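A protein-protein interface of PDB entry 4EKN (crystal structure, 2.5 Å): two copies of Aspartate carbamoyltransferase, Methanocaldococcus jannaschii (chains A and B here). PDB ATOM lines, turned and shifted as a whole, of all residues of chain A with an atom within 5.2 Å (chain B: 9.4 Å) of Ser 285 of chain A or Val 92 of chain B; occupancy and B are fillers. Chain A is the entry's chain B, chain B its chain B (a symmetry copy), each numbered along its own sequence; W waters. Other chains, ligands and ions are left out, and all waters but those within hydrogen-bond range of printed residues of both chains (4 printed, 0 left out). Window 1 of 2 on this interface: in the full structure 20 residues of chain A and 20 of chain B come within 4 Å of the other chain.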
ATOM      1  N   LEU A 263       8.921   3.558   9.674  1.00  0.00           N
ATOM      2  CA  LEU A 263       9.655   3.266  10.909  1.00  0.00           C
ATOM      3  C   LEU A 263       9.091   2.042  11.632  1.00  0.00           C
ATOM      4  O   LEU A 263       7.925   1.690  11.447  1.00  0.00           O
ATOM      5  CB  LEU A 263       9.682   4.489  11.836  1.00  0.00           C
ATOM      6  CG  LEU A 263      10.386   5.730  11.274  1.00  0.00           C
ATOM      7  CD1 LEU A 263      10.388   6.868  12.282  1.00  0.00           C
ATOM      8  CD2 LEU A 263      11.806   5.389  10.845  1.00  0.00           C
ATOM      9  N   LYS A 280      13.287  12.661   5.265  1.00  0.00           N
ATOM     10  CA  LYS A 280      12.090  13.251   5.853  1.00  0.00           C
ATOM     11  C   LYS A 280      11.298  12.309   6.764  1.00  0.00           C
ATOM     12  O   LYS A 280      10.256  12.693   7.291  1.00  0.00           O
ATOM     13  CB  LYS A 280      11.174  13.790   4.753  1.00  0.00           C
ATOM     14  CG  LYS A 280      11.641  15.105   4.152  1.00  0.00           C
ATOM     15  CD  LYS A 280      11.423  16.257   5.120  1.00  0.00           C
ATOM     16  CE  LYS A 280      12.437  17.368   4.891  1.00  0.00           C
ATOM     17  NZ  LYS A 280      12.532  17.764   3.458  1.00  0.00           N
ATOM     18  N   TYR A 281      11.791  11.087   6.952  1.00  0.00           N
ATOM     19  CA  TYR A 281      11.067  10.082   7.733  1.00  0.00           C
ATOM     20  C   TYR A 281      10.868  10.450   9.208  1.00  0.00           C
ATOM     21  O   TYR A 281       9.892  10.035   9.834  1.00  0.00           O
ATOM     22  CB  TYR A 281      11.729   8.704   7.609  1.00  0.00           C
ATOM     23  CG  TYR A 281      13.230   8.744   7.435  1.00  0.00           C
ATOM     24  CD1 TYR A 281      13.801   8.780   6.168  1.00  0.00           C
ATOM     25  CD2 TYR A 281      14.078   8.740   8.537  1.00  0.00           C
ATOM     26  CE1 TYR A 281      15.173   8.814   6.001  1.00  0.00           C
ATOM     27  CE2 TYR A 281      15.453   8.771   8.380  1.00  0.00           C
ATOM     28  CZ  TYR A 281      15.994   8.808   7.108  1.00  0.00           C
ATOM     29  OH  TYR A 281      17.360   8.844   6.946  1.00  0.00           O
ATOM     30  N   PHE A 282      11.786  11.226   9.767  1.00  0.00           N
ATOM     31  CA  PHE A 282      11.621  11.666  11.148  1.00  0.00           C
ATOM     32  C   PHE A 282      10.609  12.802  11.256  1.00  0.00           C
ATOM     33  O   PHE A 282       9.869  12.894  12.233  1.00  0.00           O
ATOM     34  CB  PHE A 282      12.960  12.048  11.767  1.00  0.00           C
ATOM     35  CG  PHE A 282      13.823  10.864  12.101  1.00  0.00           C
ATOM     36  CD1 PHE A 282      13.402   9.934  13.037  1.00  0.00           C
ATOM     37  CD2 PHE A 282      15.047  10.680  11.481  1.00  0.00           C
ATOM     38  CE1 PHE A 282      14.187   8.842  13.348  1.00  0.00           C
ATOM     39  CE2 PHE A 282      15.837   9.591  11.791  1.00  0.00           C
ATOM     40  CZ  PHE A 282      15.406   8.671  12.727  1.00  0.00           C
ATOM     41  N   LYS A 283      10.581  13.660  10.240  1.00  0.00           N
ATOM     42  CA  LYS A 283       9.554  14.685  10.131  1.00  0.00           C
ATOM     43  C   LYS A 283       8.214  13.997   9.901  1.00  0.00           C
ATOM     44  O   LYS A 283       7.188  14.399  10.454  1.00  0.00           O
ATOM     45  CB  LYS A 283       9.876  15.643   8.977  1.00  0.00           C
ATOM     46  CG  LYS A 283       8.757  16.610   8.626  1.00  0.00           C
ATOM     47  CD  LYS A 283       8.733  17.811   9.557  1.00  0.00           C
ATOM     48  CE  LYS A 283       9.568  18.961   9.009  1.00  0.00           C
ATOM     49  NZ  LYS A 283       8.960  19.569   7.787  1.00  0.00           N
ATOM     50  N   GLN A 284       8.244  12.951   9.077  1.00  0.00           N
ATOM     51  CA  GLN A 284       7.074  12.120   8.806  1.00  0.00           C
ATOM     52  C   GLN A 284       6.494  11.593  10.114  1.00  0.00           C
ATOM     53  O   GLN A 284       5.286  11.660  10.348  1.00  0.00           O
ATOM     54  CB  GLN A 284       7.474  10.957   7.900  1.00  0.00           C
ATOM     55  CG  GLN A 284       6.398   9.914   7.631  1.00  0.00           C
ATOM     56  CD  GLN A 284       6.952   8.751   6.823  1.00  0.00           C
ATOM     57  OE1 GLN A 284       8.147   8.711   6.527  1.00  0.00           O
ATOM     58  NE2 GLN A 284       6.093   7.801   6.467  1.00  0.00           N
ATOM     59  N   SER A 285       7.374  11.074  10.964  1.00  0.00           N
ATOM     60  CA  SER A 285       7.002  10.623  12.299  1.00  0.00           C
ATOM     61  C   SER A 285       6.242  11.694  13.076  1.00  0.00           C
ATOM     62  O   SER A 285       5.189  11.425  13.654  1.00  0.00           O
ATOM     63  CB  SER A 285       8.253  10.214  13.083  1.00  0.00           C
ATOM     64  OG  SER A 285       7.940   9.955  14.438  1.00  0.00           O
ATOM     65  N   PHE A 286       6.781  12.909  13.097  1.00  0.00           N
ATOM     66  CA  PHE A 286       6.119  14.002  13.798  1.00  0.00           C
ATOM     67  C   PHE A 286       4.724  14.267  13.232  1.00  0.00           C
ATOM     68  O   PHE A 286       3.760  14.406  13.985  1.00  0.00           O
ATOM     69  CB  PHE A 286       6.956  15.280  13.752  1.00  0.00           C
ATOM     70  CG  PHE A 286       6.193  16.505  14.161  1.00  0.00           C
ATOM     71  CD1 PHE A 286       5.909  16.747  15.494  1.00  0.00           C
ATOM     72  CD2 PHE A 286       5.745  17.406  13.213  1.00  0.00           C
ATOM     73  CE1 PHE A 286       5.198  17.871  15.874  1.00  0.00           C
ATOM     74  CE2 PHE A 286       5.035  18.531  13.586  1.00  0.00           C
ATOM     75  CZ  PHE A 286       4.762  18.763  14.917  1.00  0.00           C
ATOM     76  N   TYR A 287       4.623  14.332  11.906  1.00  0.00           N
ATOM     77  CA  TYR A 287       3.343  14.555  11.243  1.00  0.00           C
ATOM     78  C   TYR A 287       2.285  13.563  11.714  1.00  0.00           C
ATOM     79  O   TYR A 287       1.091  13.843  11.653  1.00  0.00           O
ATOM     80  CB  TYR A 287       3.501  14.466   9.724  1.00  0.00           C
ATOM     81  CG  TYR A 287       4.153  15.679   9.107  1.00  0.00           C
ATOM     82  CD1 TYR A 287       4.058  16.927   9.714  1.00  0.00           C
ATOM     83  CD2 TYR A 287       4.866  15.577   7.920  1.00  0.00           C
ATOM     84  CE1 TYR A 287       4.649  18.042   9.147  1.00  0.00           C
ATOM     85  CE2 TYR A 287       5.462  16.687   7.347  1.00  0.00           C
ATOM     86  CZ  TYR A 287       5.350  17.915   7.965  1.00  0.00           C
ATOM     87  OH  TYR A 287       5.944  19.018   7.400  1.00  0.00           O
ATOM     88  N   GLY A 288       2.730  12.401  12.176  1.00  0.00           N
ATOM     89  CA  GLY A 288       1.822  11.390  12.677  1.00  0.00           C
ATOM     90  C   GLY A 288       0.973  11.896  13.829  1.00  0.00           C
ATOM     91  O   GLY A 288      -0.149  11.436  14.030  1.00  0.00           O
ATOM     92  N   ILE A 289       1.506  12.851  14.586  1.00  0.00           N
ATOM     93  CA  ILE A 289       0.798  13.375  15.752  1.00  0.00           C
ATOM     94  C   ILE A 289      -0.379  14.287  15.383  1.00  0.00           C
ATOM     95  O   ILE A 289      -1.487  14.091  15.882  1.00  0.00           O
ATOM     96  CB  ILE A 289       1.751  14.096  16.730  1.00  0.00           C
ATOM     97  CG1 ILE A 289       2.831  13.135  17.225  1.00  0.00           C
ATOM     98  CG2 ILE A 289       0.973  14.672  17.907  1.00  0.00           C
ATOM     99  CD1 ILE A 289       2.287  11.951  17.998  1.00  0.00           C
ATOM    100  N   ALA B  44       8.360  12.487  28.476  1.00  0.00           N
ATOM    101  CA  ALA B  44       8.501  11.132  27.966  1.00  0.00           C
ATOM    102  C   ALA B  44       9.483  10.341  28.817  1.00  0.00           C
ATOM    103  O   ALA B  44      10.660  10.696  28.922  1.00  0.00           O
ATOM    104  CB  ALA B  44       8.944  11.149  26.510  1.00  0.00           C
ATOM    105  N   VAL B  46      11.667   7.292  29.099  1.00  0.00           N
ATOM    106  CA  VAL B  46      12.300   6.332  28.206  1.00  0.00           C
ATOM    107  C   VAL B  46      13.324   5.474  28.938  1.00  0.00           C
ATOM    108  O   VAL B  46      14.448   5.900  29.198  1.00  0.00           O
ATOM    109  CB  VAL B  46      12.966   7.032  27.010  1.00  0.00           C
ATOM    110  CG1 VAL B  46      13.569   6.005  26.063  1.00  0.00           C
ATOM    111  CG2 VAL B  46      11.949   7.898  26.281  1.00  0.00           C
ATOM    112  N   ILE B  70       4.001  10.380  28.932  1.00  0.00           N
ATOM    113  CA  ILE B  70       3.948   9.135  28.169  1.00  0.00           C
ATOM    114  C   ILE B  70       5.102   8.239  28.608  1.00  0.00           C
ATOM    115  O   ILE B  70       6.185   8.729  28.926  1.00  0.00           O
ATOM    116  CB  ILE B  70       4.011   9.368  26.644  1.00  0.00           C
ATOM    117  CG1 ILE B  70       5.339  10.023  26.254  1.00  0.00           C
ATOM    118  CG2 ILE B  70       2.830  10.211  26.177  1.00  0.00           C
ATOM    119  CD1 ILE B  70       5.495  10.236  24.764  1.00  0.00           C
ATOM    120  N   MET B  72       7.617   4.637  28.334  1.00  0.00           N
ATOM    121  CA  MET B  72       8.257   3.628  27.497  1.00  0.00           C
ATOM    122  C   MET B  72       9.333   2.945  28.337  1.00  0.00           C
ATOM    123  O   MET B  72      10.471   3.413  28.392  1.00  0.00           O
ATOM    124  CB  MET B  72       8.883   4.298  26.275  1.00  0.00           C
ATOM    125  CG  MET B  72       9.231   3.364  25.130  1.00  0.00           C
ATOM    126  SD  MET B  72       9.953   4.278  23.751  1.00  0.00           S
ATOM    127  CE  MET B  72       9.841   3.074  22.429  1.00  0.00           C
ATOM    128  N   GLU B  84      15.287  -0.840  16.201  1.00  0.00           N
ATOM    129  CA  GLU B  84      15.537   0.594  16.322  1.00  0.00           C
ATOM    130  C   GLU B  84      16.678   0.905  17.288  1.00  0.00           C
ATOM    131  O   GLU B  84      16.674   0.453  18.430  1.00  0.00           O
ATOM    132  CB  GLU B  84      14.262   1.309  16.766  1.00  0.00           C
ATOM    133  CG  GLU B  84      14.261   2.803  16.516  1.00  0.00           C
ATOM    134  CD  GLU B  84      12.889   3.420  16.717  1.00  0.00           C
ATOM    135  OE1 GLU B  84      12.545   3.757  17.869  1.00  0.00           O
ATOM    136  OE2 GLU B  84      12.153   3.562  15.720  1.00  0.00           O
ATOM    137  N   SER B  85      17.655   1.678  16.823  1.00  0.00           N
ATOM    138  CA  SER B  85      18.763   2.096  17.673  1.00  0.00           C
ATOM    139  C   SER B  85      18.313   3.200  18.622  1.00  0.00           C
ATOM    140  O   SER B  85      17.264   3.809  18.425  1.00  0.00           O
ATOM    141  CB  SER B  85      19.940   2.593  16.834  1.00  0.00           C
ATOM    142  OG  SER B  85      19.676   3.879  16.299  1.00  0.00           O
ATOM    143  N   LEU B  86      19.117   3.458  19.644  1.00  0.00           N
ATOM    144  CA  LEU B  86      18.806   4.495  20.620  1.00  0.00           C
ATOM    145  C   LEU B  86      18.554   5.844  19.951  1.00  0.00           C
ATOM    146  O   LEU B  86      17.535   6.485  20.206  1.00  0.00           O
ATOM    147  CB  LEU B  86      19.932   4.613  21.648  1.00  0.00           C
ATOM    148  CG  LEU B  86      19.831   5.731  22.683  1.00  0.00           C
ATOM    149  CD1 LEU B  86      18.499   5.681  23.412  1.00  0.00           C
ATOM    150  CD2 LEU B  86      20.984   5.642  23.669  1.00  0.00           C
ATOM    151  N   ILE B  87      19.476   6.268  19.091  1.00  0.00           N
ATOM    152  CA  ILE B  87      19.382   7.590  18.464  1.00  0.00           C
ATOM    153  C   ILE B  87      18.113   7.770  17.635  1.00  0.00           C
ATOM    154  O   ILE B  87      17.631   8.890  17.475  1.00  0.00           O
ATOM    155  CB  ILE B  87      20.607   7.914  17.574  1.00  0.00           C
ATOM    156  CG1 ILE B  87      20.705   6.930  16.408  1.00  0.00           C
ATOM    157  CG2 ILE B  87      21.888   7.933  18.396  1.00  0.00           C
ATOM    158  CD1 ILE B  87      21.723   7.331  15.367  1.00  0.00           C
ATOM    159  N   ASP B  88      17.583   6.675  17.100  1.00  0.00           N
ATOM    160  CA  ASP B  88      16.326   6.733  16.358  1.00  0.00           C
ATOM    161  C   ASP B  88      15.158   6.976  17.306  1.00  0.00           C
ATOM    162  O   ASP B  88      14.317   7.839  17.060  1.00  0.00           O
ATOM    163  CB  ASP B  88      16.092   5.442  15.568  1.00  0.00           C
ATOM    164  CG  ASP B  88      16.656   5.504  14.164  1.00  0.00           C
ATOM    165  OD1 ASP B  88      17.511   6.378  13.901  1.00  0.00           O
ATOM    166  OD2 ASP B  88      16.243   4.679  13.324  1.00  0.00           O
ATOM    167  N   THR B  89      15.115   6.206  18.387  1.00  0.00           N
ATOM    168  CA  THR B  89      14.041   6.314  19.362  1.00  0.00           C
ATOM    169  C   THR B  89      14.001   7.708  19.972  1.00  0.00           C
ATOM    170  O   THR B  89      12.934   8.304  20.119  1.00  0.00           O
ATOM    171  CB  THR B  89      14.201   5.286  20.488  1.00  0.00           C
ATOM    172  OG1 THR B  89      14.154   3.964  19.937  1.00  0.00           O
ATOM    173  CG2 THR B  89      13.091   5.447  21.514  1.00  0.00           C
ATOM    174  N   ILE B  90      15.176   8.217  20.326  1.00  0.00           N
ATOM    175  CA  ILE B  90      15.301   9.553  20.887  1.00  0.00           C
ATOM    176  C   ILE B  90      14.712  10.597  19.939  1.00  0.00           C
ATOM    177  O   ILE B  90      13.949  11.467  20.356  1.00  0.00           O
ATOM    178  CB  ILE B  90      16.775   9.890  21.199  1.00  0.00           C
ATOM    179  CG1 ILE B  90      17.279   9.038  22.368  1.00  0.00           C
ATOM    180  CG2 ILE B  90      16.933  11.365  21.522  1.00  0.00           C
ATOM    181  CD1 ILE B  90      16.641   9.384  23.704  1.00  0.00           C
ATOM    182  N   ARG B  91      15.058  10.497  18.660  1.00  0.00           N
ATOM    183  CA  ARG B  91      14.567  11.440  17.661  1.00  0.00           C
ATOM    184  C   ARG B  91      13.052  11.375  17.492  1.00  0.00           C
ATOM    185  O   ARG B  91      12.387  12.409  17.422  1.00  0.00           O
ATOM    186  CB  ARG B  91      15.285  11.241  16.321  1.00  0.00           C
ATOM    187  CG  ARG B  91      16.677  11.874  16.291  1.00  0.00           C
ATOM    188  CD  ARG B  91      17.399  11.655  14.965  1.00  0.00           C
ATOM    189  NE  ARG B  91      17.862  10.279  14.805  1.00  0.00           N
ATOM    190  CZ  ARG B  91      18.813   9.906  13.953  1.00  0.00           C
ATOM    191  NH1 ARG B  91      19.411  10.809  13.185  1.00  0.00           N
ATOM    192  NH2 ARG B  91      19.171   8.629  13.875  1.00  0.00           N
ATOM    193  N   VAL B  92      12.503  10.166  17.434  1.00  0.00           N
ATOM    194  CA  VAL B  92      11.059  10.005  17.319  1.00  0.00           C
ATOM    195  C   VAL B  92      10.358  10.595  18.537  1.00  0.00           C
ATOM    196  O   VAL B  92       9.356  11.295  18.417  1.00  0.00           O
ATOM    197  CB  VAL B  92      10.656   8.523  17.201  1.00  0.00           C
ATOM    198  CG1 VAL B  92       9.179   8.345  17.548  1.00  0.00           C
ATOM    199  CG2 VAL B  92      10.959   7.994  15.809  1.00  0.00           C
ATOM    200  N   ILE B  93      10.908  10.310  19.710  1.00  0.00           N
ATOM    201  CA  ILE B  93      10.284  10.705  20.964  1.00  0.00           C
ATOM    202  C   ILE B  93      10.452  12.190  21.284  1.00  0.00           C
ATOM    203  O   ILE B  93       9.563  12.805  21.874  1.00  0.00           O
ATOM    204  CB  ILE B  93      10.779   9.825  22.128  1.00  0.00           C
ATOM    205  CG1 ILE B  93      10.029   8.493  22.119  1.00  0.00           C
ATOM    206  CG2 ILE B  93      10.593  10.526  23.459  1.00  0.00           C
ATOM    207  CD1 ILE B  93      10.460   7.542  23.201  1.00  0.00           C
ATOM    208  N   SER B  94      11.579  12.772  20.885  1.00  0.00           N
ATOM    209  CA  SER B  94      11.769  14.206  21.072  1.00  0.00           C
ATOM    210  C   SER B  94      10.861  14.979  20.121  1.00  0.00           C
ATOM    211  O   SER B  94      10.628  16.173  20.302  1.00  0.00           O
ATOM    212  CB  SER B  94      13.235  14.605  20.885  1.00  0.00           C
ATOM    213  OG  SER B  94      13.728  14.173  19.634  1.00  0.00           O
ATOM    214  N   GLY B  95      10.344  14.287  19.112  1.00  0.00           N
ATOM    215  CA  GLY B  95       9.352  14.864  18.220  1.00  0.00           C
ATOM    216  C   GLY B  95       7.966  14.822  18.838  1.00  0.00           C
ATOM    217  O   GLY B  95       7.149  15.722  18.625  1.00  0.00           O
ATOM    218  N   TYR B  96       7.702  13.776  19.617  1.00  0.00           N
ATOM    219  CA  TYR B  96       6.426  13.636  20.312  1.00  0.00           C
ATOM    220  C   TYR B  96       6.348  14.527  21.549  1.00  0.00           C
ATOM    221  O   TYR B  96       5.363  15.237  21.749  1.00  0.00           O
ATOM    222  CB  TYR B  96       6.201  12.183  20.745  1.00  0.00           C
ATOM    223  CG  TYR B  96       5.960  11.199  19.624  1.00  0.00           C
ATOM    224  CD1 TYR B  96       5.920  11.612  18.298  1.00  0.00           C
ATOM    225  CD2 TYR B  96       5.754   9.853  19.897  1.00  0.00           C
ATOM    226  CE1 TYR B  96       5.693  10.709  17.274  1.00  0.00           C
ATOM    227  CE2 TYR B  96       5.523   8.945  18.883  1.00  0.00           C
ATOM    228  CZ  TYR B  96       5.494   9.375  17.575  1.00  0.00           C
ATOM    229  OH  TYR B  96       5.264   8.464  16.571  1.00  0.00           O
ATOM    230  N   ALA B  97       7.387  14.479  22.379  1.00  0.00           N
ATOM    231  CA  ALA B  97       7.347  15.096  23.704  1.00  0.00           C
ATOM    232  C   ALA B  97       8.082  16.433  23.814  1.00  0.00           C
ATOM    233  O   ALA B  97       8.601  16.963  22.832  1.00  0.00           O
ATOM    234  CB  ALA B  97       7.866  14.122  24.753  1.00  0.00           C
ATOM    235  N   ASP B  98       8.121  16.965  25.032  1.00  0.00           N
ATOM    236  CA  ASP B  98       8.766  18.243  25.304  1.00  0.00           C
ATOM    237  C   ASP B  98      10.018  18.054  26.152  1.00  0.00           C
ATOM    238  O   ASP B  98      10.846  18.954  26.265  1.00  0.00           O
ATOM    239  CB  ASP B  98       7.790  19.181  26.014  1.00  0.00           C
ATOM    240  CG  ASP B  98       6.550  19.457  25.191  1.00  0.00           C
ATOM    241  OD1 ASP B  98       6.692  19.773  23.990  1.00  0.00           O
ATOM    242  OD2 ASP B  98       5.434  19.340  25.738  1.00  0.00           O
ATOM    243  N   ILE B 100      12.544  14.529  28.100  1.00  0.00           N
ATOM    244  CA  ILE B 100      12.733  13.087  28.251  1.00  0.00           C
ATOM    245  C   ILE B 100      13.553  12.717  29.481  1.00  0.00           C
ATOM    246  O   ILE B 100      14.588  13.323  29.761  1.00  0.00           O
ATOM    247  CB  ILE B 100      13.431  12.488  27.025  1.00  0.00           C
ATOM    248  CG1 ILE B 100      12.587  12.711  25.769  1.00  0.00           C
ATOM    249  CG2 ILE B 100      13.704  11.006  27.244  1.00  0.00           C
ATOM    250  CD1 ILE B 100      13.352  12.513  24.476  1.00  0.00           C
ATOM    251  N   TYR B 116      21.319  14.018  19.944  1.00  0.00           N
ATOM    252  CA  TYR B 116      20.325  13.797  18.893  1.00  0.00           C
ATOM    253  C   TYR B 116      18.928  14.263  19.291  1.00  0.00           C
ATOM    254  O   TYR B 116      17.998  14.201  18.490  1.00  0.00           O
ATOM    255  CB  TYR B 116      20.269  12.318  18.499  1.00  0.00           C
ATOM    256  CG  TYR B 116      21.485  11.842  17.746  1.00  0.00           C
ATOM    257  CD1 TYR B 116      22.669  11.565  18.412  1.00  0.00           C
ATOM    258  CD2 TYR B 116      21.449  11.668  16.372  1.00  0.00           C
ATOM    259  CE1 TYR B 116      23.784  11.131  17.731  1.00  0.00           C
ATOM    260  CE2 TYR B 116      22.560  11.232  15.681  1.00  0.00           C
ATOM    261  CZ  TYR B 116      23.727  10.966  16.366  1.00  0.00           C
ATOM    262  OH  TYR B 116      24.846  10.533  15.689  1.00  0.00           O
ATOM    263  N   SER B 117      18.778  14.724  20.528  1.00  0.00           N
ATOM    264  CA  SER B 117      17.466  15.132  21.019  1.00  0.00           C
ATOM    265  C   SER B 117      17.220  16.624  20.810  1.00  0.00           C
ATOM    266  O   SER B 117      18.083  17.456  21.092  1.00  0.00           O
ATOM    267  CB  SER B 117      17.311  14.770  22.497  1.00  0.00           C
ATOM    268  OG  SER B 117      15.999  15.041  22.955  1.00  0.00           O
ATOM    269  N   GLN B 118      16.041  16.961  20.307  1.00  0.00           N
ATOM    270  CA  GLN B 118      15.674  18.362  20.165  1.00  0.00           C
ATOM    271  C   GLN B 118      15.094  18.905  21.472  1.00  0.00           C
ATOM    272  O   GLN B 118      14.905  20.110  21.619  1.00  0.00           O
ATOM    273  CB  GLN B 118      14.706  18.566  18.990  1.00  0.00           C
ATOM    274  CG  GLN B 118      13.475  17.675  19.019  1.00  0.00           C
ATOM    275  CD  GLN B 118      12.595  17.860  17.793  1.00  0.00           C
ATOM    276  OE1 GLN B 118      11.399  18.128  17.909  1.00  0.00           O
ATOM    277  NE2 GLN B 118      13.187  17.714  16.612  1.00  0.00           N
ATOM    278  N   VAL B 119      14.831  18.010  22.421  1.00  0.00           N
ATOM    279  CA  VAL B 119      14.318  18.404  23.730  1.00  0.00           C
ATOM    280  C   VAL B 119      15.313  18.039  24.830  1.00  0.00           C
ATOM    281  O   VAL B 119      16.210  17.225  24.612  1.00  0.00           O
ATOM    282  CB  VAL B 119      12.951  17.750  24.043  1.00  0.00           C
ATOM    283  CG1 VAL B 119      11.986  17.933  22.876  1.00  0.00           C
ATOM    284  CG2 VAL B 119      13.124  16.278  24.387  1.00  0.00           C
HETATM  285  O   HOH W   1       8.356  12.056  16.077  1.00  0.00           O
HETATM  286  O   HOH W   2      10.463  13.478  14.798  1.00  0.00           O
HETATM  287  O   HOH W   3       6.647   7.198  14.307  1.00  0.00           O
HETATM  288  O   HOH W   4       3.890   9.264  14.447  1.00  0.00           O
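No position is printed for both chains.
Of the 7 pairs that touch across the chains among the printed residues, none has its exchanged pair printed and touching as well.
Leu 263 of chain A touches Val 92 of chain B (CD1 to CG2, 3.7 Å).
Asp 88 of chain B touches Phe 282 of chain A.
Arg 91 of chain B touches Phe 282 of chain A (NE to CZ, 3.6 Å).
Ser 285 of chain A touches Val 92 of chain B.
Ser 285 of chain A touches Tyr 96 of chain B (OG to CE1, 3.7 Å).
Phe 286 of chain A touches Gly 95 of chain B.
Tyr 96 of chain B touches Ile 289 of chain A (CD1 to CG1, 3.6 Å).
Printed residues of chain B within 4 Å of Phe 282 of chain A: Asp 88 and Arg 91.
Gln 284 of chain A touches none of the printed residues of chain B.
Of chain B, only Val 92 and Tyr 96 come within 4 Å of Ser 285 of chain A.
Thr 89 of chain B touches none of the printed residues of chain A.
Val 92 of chain B touches just these residues of chain A: Leu 263 and Ser 285.
Of the printed residues of chain A, Gly 95 of chain B touches Phe 286 (3.5 Å).
The nearest printed residue of chain B that does not touch Ile 289 of chain A is Gly 95 of chain B (5.2 Å).
The backbone carbonyl oxygen (O) of Ile 87 of chain B lies within hydrogen-bond range of the guanidinium group (NE) of Arg 91 of chain B, at 3.0 Å.
The side-chain carboxylate (OD1) of Asp 88 of chain B lies within salt-bridge range of the guanidinium group (NH2) of Arg 91 of chain B, at 2.8 Å.
The backbone carbonyl oxygen (O) of Arg 91 of chain B is in hydrogen-bond range of the side-chain hydroxyl (OG) of Ser 94 of chain B, 3.1 Å away.
Hydrophobic or aromatic side chains of chain A within 4 Å of the printed part of chain B: Leu 263, Phe 282, Phe 286 and Ile 289.
Hydrophobic or aromatic side chains of chain B within 4 Å of the printed part of chain A: Val 92 and Tyr 96.
Among the printed residues, 7 pairs touch across the chains.
Water W4 lies within hydrogen-bond range of O of Ser 285 of chain A (2.6 Å) and OH of Tyr 96 of chain B (2.7 Å).
Water W1 lies within hydrogen-bond range of O of Val 92 of chain B (2.7 Å), OG of Ser 285 of chain A (2.7 Å) and N of Phe 286 of chain A (3.5 Å).
Water W2 bridges the backbone carbonyl oxygen of Phe 282 of chain A (2.7 Å) and the backbone carbonyl oxygen of Arg 91 of chain B (3.4 Å).
Water W3 lies within hydrogen-bond range of OH of Tyr 96 of chain B (2.9 Å) and OG of Ser 285 of chain A (3.0 Å).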
